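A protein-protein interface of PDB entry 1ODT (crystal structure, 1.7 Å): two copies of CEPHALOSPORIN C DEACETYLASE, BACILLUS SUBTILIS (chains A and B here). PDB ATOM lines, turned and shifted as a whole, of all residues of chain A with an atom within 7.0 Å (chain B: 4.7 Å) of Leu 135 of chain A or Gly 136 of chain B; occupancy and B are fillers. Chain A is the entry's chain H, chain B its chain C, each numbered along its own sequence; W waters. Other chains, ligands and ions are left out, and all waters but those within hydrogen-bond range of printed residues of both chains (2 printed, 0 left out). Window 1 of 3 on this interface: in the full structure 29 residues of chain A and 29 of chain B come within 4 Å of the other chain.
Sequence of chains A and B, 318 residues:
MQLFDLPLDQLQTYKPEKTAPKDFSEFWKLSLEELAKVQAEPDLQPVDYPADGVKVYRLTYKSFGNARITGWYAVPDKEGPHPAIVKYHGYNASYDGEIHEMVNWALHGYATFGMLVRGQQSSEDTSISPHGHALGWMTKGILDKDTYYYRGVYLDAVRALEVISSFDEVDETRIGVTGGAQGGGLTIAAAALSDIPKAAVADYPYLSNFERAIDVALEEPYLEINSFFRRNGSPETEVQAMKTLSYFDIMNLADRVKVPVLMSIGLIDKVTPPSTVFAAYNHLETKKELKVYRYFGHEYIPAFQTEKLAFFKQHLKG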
ATOM      1  N   TYR A  91      13.421  23.273 -19.148  1.00  0.00           N
ATOM      2  CA  TYR A  91      13.400  21.963 -18.498  1.00  0.00           C
ATOM      3  C   TYR A  91      12.383  21.850 -17.362  1.00  0.00           C
ATOM      4  O   TYR A  91      12.454  22.594 -16.396  1.00  0.00           O
ATOM      5  CB  TYR A  91      14.790  21.698 -17.946  1.00  0.00           C
ATOM      6  CG  TYR A  91      15.039  20.289 -17.487  1.00  0.00           C
ATOM      7  CD1 TYR A  91      14.934  19.955 -16.154  1.00  0.00           C
ATOM      8  CD2 TYR A  91      15.419  19.303 -18.392  1.00  0.00           C
ATOM      9  CE1 TYR A  91      15.210  18.653 -15.721  1.00  0.00           C
ATOM     10  CE2 TYR A  91      15.667  17.990 -17.973  1.00  0.00           C
ATOM     11  CZ  TYR A  91      15.570  17.689 -16.626  1.00  0.00           C
ATOM     12  OH  TYR A  91      15.868  16.401 -16.185  1.00  0.00           O
ATOM     13  N   ASN A  92      11.410  20.970 -17.507  1.00  0.00           N
ATOM     14  CA  ASN A  92      10.397  20.744 -16.487  1.00  0.00           C
ATOM     15  C   ASN A  92       9.633  22.043 -16.191  1.00  0.00           C
ATOM     16  O   ASN A  92       9.107  22.187 -15.115  1.00  0.00           O
ATOM     17  CB  ASN A  92      11.085  20.239 -15.199  1.00  0.00           C
ATOM     18  CG  ASN A  92      10.092  19.728 -14.147  1.00  0.00           C
ATOM     19  OD1 ASN A  92       9.173  18.994 -14.469  1.00  0.00           O
ATOM     20  ND2 ASN A  92      10.350  20.048 -12.880  1.00  0.00           N
ATOM     21  N   GLY A 119       7.334  13.782 -22.704  1.00  0.00           N
ATOM     22  CA  GLY A 119       7.525  13.383 -21.320  1.00  0.00           C
ATOM     23  C   GLY A 119       7.496  14.469 -20.235  1.00  0.00           C
ATOM     24  O   GLY A 119       7.244  14.142 -19.074  1.00  0.00           O
ATOM     25  N   HIS A 133      18.061   5.224 -14.670  1.00  0.00           N
ATOM     26  CA  HIS A 133      18.728   6.531 -14.722  1.00  0.00           C
ATOM     27  C   HIS A 133      18.485   7.294 -13.421  1.00  0.00           C
ATOM     28  O   HIS A 133      17.568   6.944 -12.645  1.00  0.00           O
ATOM     29  CB  HIS A 133      18.272   7.339 -15.971  1.00  0.00           C
ATOM     30  CG  HIS A 133      16.778   7.512 -16.092  1.00  0.00           C
ATOM     31  ND1 HIS A 133      16.088   8.498 -15.427  1.00  0.00           N
ATOM     32  CD2 HIS A 133      15.845   6.819 -16.799  1.00  0.00           C
ATOM     33  CE1 HIS A 133      14.799   8.417 -15.731  1.00  0.00           C
ATOM     34  NE2 HIS A 133      14.632   7.421 -16.573  1.00  0.00           N
ATOM     35  N   ALA A 134      19.279   8.344 -13.177  1.00  0.00           N
ATOM     36  CA  ALA A 134      19.015   9.260 -12.070  1.00  0.00           C
ATOM     37  C   ALA A 134      17.689   9.993 -12.300  1.00  0.00           C
ATOM     38  O   ALA A 134      17.234  10.155 -13.439  1.00  0.00           O
ATOM     39  CB  ALA A 134      20.123  10.253 -11.930  1.00  0.00           C
ATOM     40  N   LEU A 135      17.097  10.440 -11.208  1.00  0.00           N
ATOM     41  CA  LEU A 135      15.824  11.187 -11.218  1.00  0.00           C
ATOM     42  C   LEU A 135      15.908  12.340 -12.220  1.00  0.00           C
ATOM     43  O   LEU A 135      16.814  13.179 -12.155  1.00  0.00           O
ATOM     44  CB  LEU A 135      15.567  11.737  -9.810  1.00  0.00           C
ATOM     45  CG  LEU A 135      14.268  12.486  -9.513  1.00  0.00           C
ATOM     46  CD1 LEU A 135      13.214  11.569  -9.643  1.00  0.00           C
ATOM     47  CD2 LEU A 135      14.305  13.006  -8.054  1.00  0.00           C
ATOM     48  N   GLY A 136      14.966  12.356 -13.153  1.00  0.00           N
ATOM     49  CA  GLY A 136      14.957  13.318 -14.244  1.00  0.00           C
ATOM     50  C   GLY A 136      15.089  12.675 -15.605  1.00  0.00           C
ATOM     51  O   GLY A 136      14.996  11.470 -15.761  1.00  0.00           O
ATOM     52  N   TRP A 137      15.264  13.510 -16.615  1.00  0.00           N
ATOM     53  CA  TRP A 137      15.356  13.082 -17.995  1.00  0.00           C
ATOM     54  C   TRP A 137      16.786  13.118 -18.499  1.00  0.00           C
ATOM     55  O   TRP A 137      17.066  12.573 -19.551  1.00  0.00           O
ATOM     56  CB  TRP A 137      14.509  14.016 -18.905  1.00  0.00           C
ATOM     57  CG  TRP A 137      12.999  13.859 -18.672  1.00  0.00           C
ATOM     58  CD1 TRP A 137      12.191  12.922 -19.215  1.00  0.00           C
ATOM     59  CD2 TRP A 137      12.174  14.691 -17.873  1.00  0.00           C
ATOM     60  NE1 TRP A 137      10.894  13.090 -18.774  1.00  0.00           N
ATOM     61  CE2 TRP A 137      10.863  14.202 -17.971  1.00  0.00           C
ATOM     62  CE3 TRP A 137      12.405  15.814 -17.078  1.00  0.00           C
ATOM     63  CZ2 TRP A 137       9.804  14.775 -17.263  1.00  0.00           C
ATOM     64  CZ3 TRP A 137      11.358  16.401 -16.408  1.00  0.00           C
ATOM     65  CH2 TRP A 137      10.082  15.864 -16.479  1.00  0.00           C
ATOM     66  N   MET A 138      17.674  13.828 -17.818  1.00  0.00           N
ATOM     67  CA  MET A 138      19.019  14.093 -18.391  1.00  0.00           C
ATOM     68  C   MET A 138      19.848  12.854 -18.659  1.00  0.00           C
ATOM     69  O   MET A 138      20.759  12.886 -19.500  1.00  0.00           O
ATOM     70  CB  MET A 138      19.877  14.980 -17.438  1.00  0.00           C
ATOM     71  CG  MET A 138      19.412  16.435 -17.308  1.00  0.00           C
ATOM     72  SD  MET A 138      19.205  17.272 -18.864  1.00  0.00           S
ATOM     73  CE  MET A 138      20.877  17.306 -19.494  1.00  0.00           C
ATOM     74  N   THR A 139      19.603  11.781 -17.895  1.00  0.00           N
ATOM     75  CA  THR A 139      20.371  10.553 -18.031  1.00  0.00           C
ATOM     76  C   THR A 139      19.566   9.387 -18.564  1.00  0.00           C
ATOM     77  O   THR A 139      20.038   8.232 -18.625  1.00  0.00           O
ATOM     78  CB  THR A 139      21.138  10.173 -16.751  1.00  0.00           C
ATOM     79  OG1 THR A 139      20.260  10.015 -15.627  1.00  0.00           O
ATOM     80  CG2 THR A 139      22.035  11.293 -16.356  1.00  0.00           C
ATOM     81  N   GLU A 220      20.638  22.307 -10.217  1.00  0.00           N
ATOM     82  CA  GLU A 220      20.047  21.410 -11.200  1.00  0.00           C
ATOM     83  C   GLU A 220      19.781  22.149 -12.515  1.00  0.00           C
ATOM     84  O   GLU A 220      19.578  23.382 -12.487  1.00  0.00           O
ATOM     85  CB  GLU A 220      18.722  20.864 -10.640  1.00  0.00           C
ATOM     86  CG  GLU A 220      18.865  20.111  -9.360  1.00  0.00           C
ATOM     87  CD  GLU A 220      19.775  18.918  -9.511  1.00  0.00           C
ATOM     88  OE1 GLU A 220      19.649  18.222 -10.539  1.00  0.00           O
ATOM     89  OE2 GLU A 220      20.601  18.687  -8.599  1.00  0.00           O
ATOM     90  N   PRO A 221      19.642  21.455 -13.649  1.00  0.00           N
ATOM     91  CA  PRO A 221      19.655  20.002 -13.754  1.00  0.00           C
ATOM     92  C   PRO A 221      20.898  19.392 -14.408  1.00  0.00           C
ATOM     93  O   PRO A 221      20.861  18.189 -14.644  1.00  0.00           O
ATOM     94  CB  PRO A 221      18.427  19.744 -14.671  1.00  0.00           C
ATOM     95  CG  PRO A 221      18.141  21.081 -15.373  1.00  0.00           C
ATOM     96  CD  PRO A 221      19.229  22.041 -14.937  1.00  0.00           C
ATOM     97  N   GLU A 224      22.133  16.253 -12.532  1.00  0.00           N
ATOM     98  CA  GLU A 224      21.573  14.904 -12.725  1.00  0.00           C
ATOM     99  C   GLU A 224      22.604  13.926 -13.267  1.00  0.00           C
ATOM    100  O   GLU A 224      22.535  12.744 -12.973  1.00  0.00           O
ATOM    101  CB  GLU A 224      20.354  14.923 -13.671  1.00  0.00           C
ATOM    102  CG  GLU A 224      19.097  15.563 -13.100  1.00  0.00           C
ATOM    103  CD  GLU A 224      17.958  15.526 -14.082  1.00  0.00           C
ATOM    104  OE1 GLU A 224      18.041  14.647 -14.976  1.00  0.00           O
ATOM    105  OE2 GLU A 224      17.017  16.368 -13.945  1.00  0.00           O
ATOM    106  N   SER A 227      24.649  12.874 -10.496  1.00  0.00           N
ATOM    107  CA  SER A 227      23.898  11.953  -9.688  1.00  0.00           C
ATOM    108  C   SER A 227      23.910  10.539 -10.280  1.00  0.00           C
ATOM    109  O   SER A 227      23.990   9.548  -9.540  1.00  0.00           O
ATOM    110  CB  SER A 227      22.459  12.412  -9.507  1.00  0.00           C
ATOM    111  OG  SER A 227      22.435  13.648  -8.795  1.00  0.00           O
ATOM    112  N   PHE A 228      23.836  10.462 -11.600  1.00  0.00           N
ATOM    113  CA  PHE A 228      23.869   9.199 -12.308  1.00  0.00           C
ATOM    114  C   PHE A 228      25.244   8.535 -12.111  1.00  0.00           C
ATOM    115  O   PHE A 228      25.324   7.336 -11.843  1.00  0.00           O
ATOM    116  CB  PHE A 228      23.599   9.436 -13.793  1.00  0.00           C
ATOM    117  CG  PHE A 228      23.665   8.196 -14.646  1.00  0.00           C
ATOM    118  CD1 PHE A 228      22.641   7.289 -14.656  1.00  0.00           C
ATOM    119  CD2 PHE A 228      24.731   7.994 -15.484  1.00  0.00           C
ATOM    120  CE1 PHE A 228      22.690   6.165 -15.455  1.00  0.00           C
ATOM    121  CE2 PHE A 228      24.792   6.884 -16.274  1.00  0.00           C
ATOM    122  CZ  PHE A 228      23.763   5.963 -16.253  1.00  0.00           C
ATOM    123  N   ARG A 231      25.399   6.887  -8.749  1.00  0.00           N
ATOM    124  CA  ARG A 231      24.567   5.664  -8.678  1.00  0.00           C
ATOM    125  C   ARG A 231      25.036   4.535  -9.590  1.00  0.00           C
ATOM    126  O   ARG A 231      24.612   3.378  -9.423  1.00  0.00           O
ATOM    127  CB  ARG A 231      23.121   5.978  -9.015  1.00  0.00           C
ATOM    128  CG  ARG A 231      22.460   6.828  -7.962  1.00  0.00           C
ATOM    129  CD  ARG A 231      21.233   7.563  -8.465  1.00  0.00           C
ATOM    130  NE  ARG A 231      20.545   8.154  -7.333  1.00  0.00           N
ATOM    131  CZ  ARG A 231      21.026   9.191  -6.669  1.00  0.00           C
ATOM    132  NH1 ARG A 231      22.141   9.775  -7.068  1.00  0.00           N
ATOM    133  NH2 ARG A 231      20.367   9.693  -5.638  1.00  0.00           N
ATOM    134  N   TYR B  91      13.316   5.097  -3.179  1.00  0.00           N
ATOM    135  CA  TYR B  91      13.092   5.933  -4.352  1.00  0.00           C
ATOM    136  C   TYR B  91      14.371   6.604  -4.772  1.00  0.00           C
ATOM    137  O   TYR B  91      14.976   7.370  -4.032  1.00  0.00           O
ATOM    138  CB  TYR B  91      12.043   6.982  -4.017  1.00  0.00           C
ATOM    139  CG  TYR B  91      11.523   7.747  -5.210  1.00  0.00           C
ATOM    140  CD1 TYR B  91      12.039   8.981  -5.518  1.00  0.00           C
ATOM    141  CD2 TYR B  91      10.468   7.260  -5.990  1.00  0.00           C
ATOM    142  CE1 TYR B  91      11.557   9.734  -6.589  1.00  0.00           C
ATOM    143  CE2 TYR B  91       9.948   8.009  -7.047  1.00  0.00           C
ATOM    144  CZ  TYR B  91      10.529   9.232  -7.363  1.00  0.00           C
ATOM    145  OH  TYR B  91      10.064  10.011  -8.379  1.00  0.00           O
ATOM    146  N   ASN B  92      14.834   6.272  -5.962  1.00  0.00           N
ATOM    147  CA  ASN B  92      16.002   6.935  -6.566  1.00  0.00           C
ATOM    148  C   ASN B  92      17.261   6.752  -5.683  1.00  0.00           C
ATOM    149  O   ASN B  92      18.176   7.555  -5.745  1.00  0.00           O
ATOM    150  CB  ASN B  92      15.745   8.457  -6.741  1.00  0.00           C
ATOM    151  CG  ASN B  92      16.838   9.187  -7.547  1.00  0.00           C
ATOM    152  OD1 ASN B  92      17.241   8.747  -8.622  1.00  0.00           O
ATOM    153  ND2 ASN B  92      17.278  10.359  -7.037  1.00  0.00           N
ATOM    154  N   HIS B 133       4.844  14.511 -17.606  1.00  0.00           N
ATOM    155  CA  HIS B 133       4.711  14.452 -16.169  1.00  0.00           C
ATOM    156  C   HIS B 133       5.768  15.329 -15.519  1.00  0.00           C
ATOM    157  O   HIS B 133       6.742  15.730 -16.150  1.00  0.00           O
ATOM    158  CB  HIS B 133       4.832  12.970 -15.694  1.00  0.00           C
ATOM    159  CG  HIS B 133       6.147  12.328 -16.011  1.00  0.00           C
ATOM    160  ND1 HIS B 133       6.318  11.457 -17.067  1.00  0.00           N
ATOM    161  CD2 HIS B 133       7.356  12.438 -15.424  1.00  0.00           C
ATOM    162  CE1 HIS B 133       7.568  11.057 -17.110  1.00  0.00           C
ATOM    163  NE2 HIS B 133       8.228  11.634 -16.124  1.00  0.00           N
ATOM    164  N   ALA B 134       5.563  15.598 -14.238  1.00  0.00           N
ATOM    165  CA  ALA B 134       6.553  16.302 -13.454  1.00  0.00           C
ATOM    166  C   ALA B 134       7.837  15.495 -13.304  1.00  0.00           C
ATOM    167  O   ALA B 134       7.830  14.253 -13.333  1.00  0.00           O
ATOM    168  CB  ALA B 134       5.996  16.688 -12.099  1.00  0.00           C
ATOM    169  N   LEU B 135       8.933  16.230 -13.151  1.00  0.00           N
ATOM    170  CA  LEU B 135      10.272  15.668 -12.863  1.00  0.00           C
ATOM    171  C   LEU B 135      10.160  14.543 -11.847  1.00  0.00           C
ATOM    172  O   LEU B 135       9.661  14.726 -10.739  1.00  0.00           O
ATOM    173  CB  LEU B 135      11.179  16.749 -12.296  1.00  0.00           C
ATOM    174  CG  LEU B 135      12.687  16.484 -12.203  1.00  0.00           C
ATOM    175  CD1 LEU B 135      13.188  16.018 -13.443  1.00  0.00           C
ATOM    176  CD2 LEU B 135      13.427  17.809 -11.850  1.00  0.00           C
ATOM    177  N   GLY B 136      10.610  13.371 -12.263  1.00  0.00           N
ATOM    178  CA  GLY B 136      10.532  12.159 -11.485  1.00  0.00           C
ATOM    179  C   GLY B 136       9.620  11.084 -12.043  1.00  0.00           C
ATOM    180  O   GLY B 136       9.179  11.134 -13.201  1.00  0.00           O
ATOM    181  N   TRP B 137       9.372  10.082 -11.219  1.00  0.00           N
ATOM    182  CA  TRP B 137       8.585   8.919 -11.638  1.00  0.00           C
ATOM    183  C   TRP B 137       7.187   8.935 -11.024  1.00  0.00           C
ATOM    184  O   TRP B 137       6.303   8.233 -11.500  1.00  0.00           O
ATOM    185  CB  TRP B 137       9.277   7.581 -11.264  1.00  0.00           C
ATOM    186  CG  TRP B 137      10.564   7.307 -11.967  1.00  0.00           C
ATOM    187  CD1 TRP B 137      10.711   6.707 -13.187  1.00  0.00           C
ATOM    188  CD2 TRP B 137      11.910   7.580 -11.495  1.00  0.00           C
ATOM    189  NE1 TRP B 137      12.052   6.669 -13.529  1.00  0.00           N
ATOM    190  CE2 TRP B 137      12.805   7.176 -12.509  1.00  0.00           C
ATOM    191  CE3 TRP B 137      12.432   8.129 -10.332  1.00  0.00           C
ATOM    192  CZ2 TRP B 137      14.177   7.290 -12.379  1.00  0.00           C
ATOM    193  CZ3 TRP B 137      13.804   8.240 -10.193  1.00  0.00           C
ATOM    194  CH2 TRP B 137      14.661   7.840 -11.214  1.00  0.00           C
ATOM    195  N   MET B 138       6.949   9.742 -10.004  1.00  0.00           N
ATOM    196  CA  MET B 138       5.695   9.649  -9.270  1.00  0.00           C
ATOM    197  C   MET B 138       4.440   9.957 -10.106  1.00  0.00           C
ATOM    198  O   MET B 138       3.355   9.508  -9.779  1.00  0.00           O
ATOM    199  CB  MET B 138       5.697  10.604  -8.068  1.00  0.00           C
ATOM    200  CG  MET B 138       6.657  10.249  -6.974  1.00  0.00           C
ATOM    201  SD  MET B 138       6.435   8.609  -6.335  1.00  0.00           S
ATOM    202  CE  MET B 138       4.825   8.549  -5.758  1.00  0.00           C
ATOM    203  N   GLU B 224       6.192  15.635  -5.754  1.00  0.00           N
ATOM    204  CA  GLU B 224       6.124  15.572  -7.206  1.00  0.00           C
ATOM    205  C   GLU B 224       4.676  15.606  -7.699  1.00  0.00           C
ATOM    206  O   GLU B 224       4.374  16.120  -8.790  1.00  0.00           O
ATOM    207  CB  GLU B 224       6.773  14.273  -7.727  1.00  0.00           C
ATOM    208  CG  GLU B 224       8.286  14.159  -7.619  1.00  0.00           C
ATOM    209  CD  GLU B 224       8.818  12.862  -8.154  1.00  0.00           C
ATOM    210  OE1 GLU B 224       8.141  12.223  -9.000  1.00  0.00           O
ATOM    211  OE2 GLU B 224       9.971  12.502  -7.794  1.00  0.00           O
HETATM  212  O   HOH W   1       7.403  18.952 -16.460  1.00  0.00           O
HETATM  213  O   HOH W   2      18.112   6.329  -9.480  1.00  0.00           O
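Water W1 bridges OD1 of Asn 92 of chain A (2.7 Å) and O of His 133 of chain B (3.3 Å).
Water W2 lies within hydrogen-bond range of OD1 of Asn 92 of chain B and O of His 133 of chain A.
OH of Tyr 91 of chain B sits at hydrogen-bond distance from N of Trp 137 of chain B (2.9 Å).
NH1 of Arg 231 of chain A sits at hydrogen-bond distance from O of Ser 227 of chain A (3.1 Å).
The backbone NH (N) of Trp 137 of chain B sits at hydrogen-bond distance from the side-chain carboxylate (OE1) of Glu 224 of chain B (3.3 Å).
OE1 of Glu 224 of chain A sits at hydrogen-bond distance from N of Trp 137 of chain A (3.4 Å).
The backbone NH (N) of Ala 134 of chain A is in hydrogen-bond range of the side-chain hydroxyl (OG1) of Thr 139 of chain A (3.1 Å).
The side-chain hydroxyl (OH) of Tyr 91 of chain B sits at hydrogen-bond distance from the side-chain carboxylate (OE2) of Glu 224 of chain B, 2.6 Å away.
Of the printed residues of chain B, Asn 92 of chain A touches Ala 134 (3.9 Å) and Leu 135 (3.1 Å).
Thr 139 of chain A touches none of the printed residues of chain B.
Of the printed residues of chain B, Arg 231 of chain A touches Asn 92.
Of the printed residues of chain A, His 133 of chain B touches Gly 119 (2.8 Å) and Trp 137 (3.4 Å).
Of the 16 printed residues of chain A, 10 touch a printed residue of chain B.
Printed residues of chain A that touch a printed residue of chain B: Tyr 91, Asn 92, Gly 119, His 133, Ala 134, Leu 135, Gly 136, Trp 137, Glu 224 and Arg 231.
Hydrophobic or aromatic side chains of chain A that line the printed part of chain B: Tyr 91, His 133, Leu 135 and Trp 137.
Printed residues of chain B that touch a printed residue of chain A: Tyr 91, Asn 92, His 133, Ala 134, Leu 135, Gly 136, Trp 137 and Glu 224.
Among the printed residues, 18 pairs touch across the chains.
Among the printed residues, no Asp or Glu carboxylate lies within 4 Å of a Lys or Arg side-chain nitrogen of the other chain.
The backbone NH (N) of Leu 135 of chain B is in hydrogen-bond range of the side-chain amide oxygen (OD1) of Asn 92 of chain A (3.1 Å).
The side-chain amide oxygen (OD1) of Asn 92 of chain B is in hydrogen-bond range of the backbone NH (N) of Leu 135 of chain A (3.1 Å).
The backbone NH (N) of His 133 of chain B sits at hydrogen-bond distance from the backbone carbonyl oxygen (O) of Gly 119 of chain A (2.8 Å).
The guanidinium group (NE) of Arg 231 of chain A sits at hydrogen-bond distance from the backbone carbonyl oxygen (O) of Asn 92 of chain B (2.9 Å).
Tyr 91 of chain A touches Leu 135 of chain B, and with the chains exchanged Leu 135 of chain A touches Tyr 91 of chain B.
His 133 of chain A touches Trp 137 of chain B, and with the chains exchanged Trp 137 of chain A touches His 133 of chain B.
Leu 135 of chain A touches Gly 136 of chain B, and with the chains exchanged Gly 136 of chain A touches Leu 135 of chain B.
Leu 135 of chain A touches Glu 224 of chain B, and with the chains exchanged Glu 224 of chain A touches Leu 135 of chain B.
Of the 18 pairs that touch across the chains among the printed residues, 16 have their exchanged pair printed and touching as well.
Tyr 91 of chain A touches Leu 135 of chain B.
Asn 92 of chain A touches Ala 134 of chain B (OD1 to CA, 3.9 Å).
C of Ala 134 of chain A touches CH2 of Trp 137 of chain B, at 3.9 Å.
Tyr 91 of chain B touches Leu 135 of chain A.
Leu 135 of chain A touches Gly 136 of chain B.
CD1 of Leu 135 of chain A touches CZ3 of Trp 137 of chain B, at 3.4 Å.
Glu 224 of chain B touches Leu 135 of chain A.
Leu 135 of chain B touches Gly 136 of chain A.
Trp 137 of chain A touches His 133 of chain B (CH2 to O, 3.4 Å).
OE2 of Glu 224 of chain A touches CD1 of Leu 135 of chain B, 3.9 Å away.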
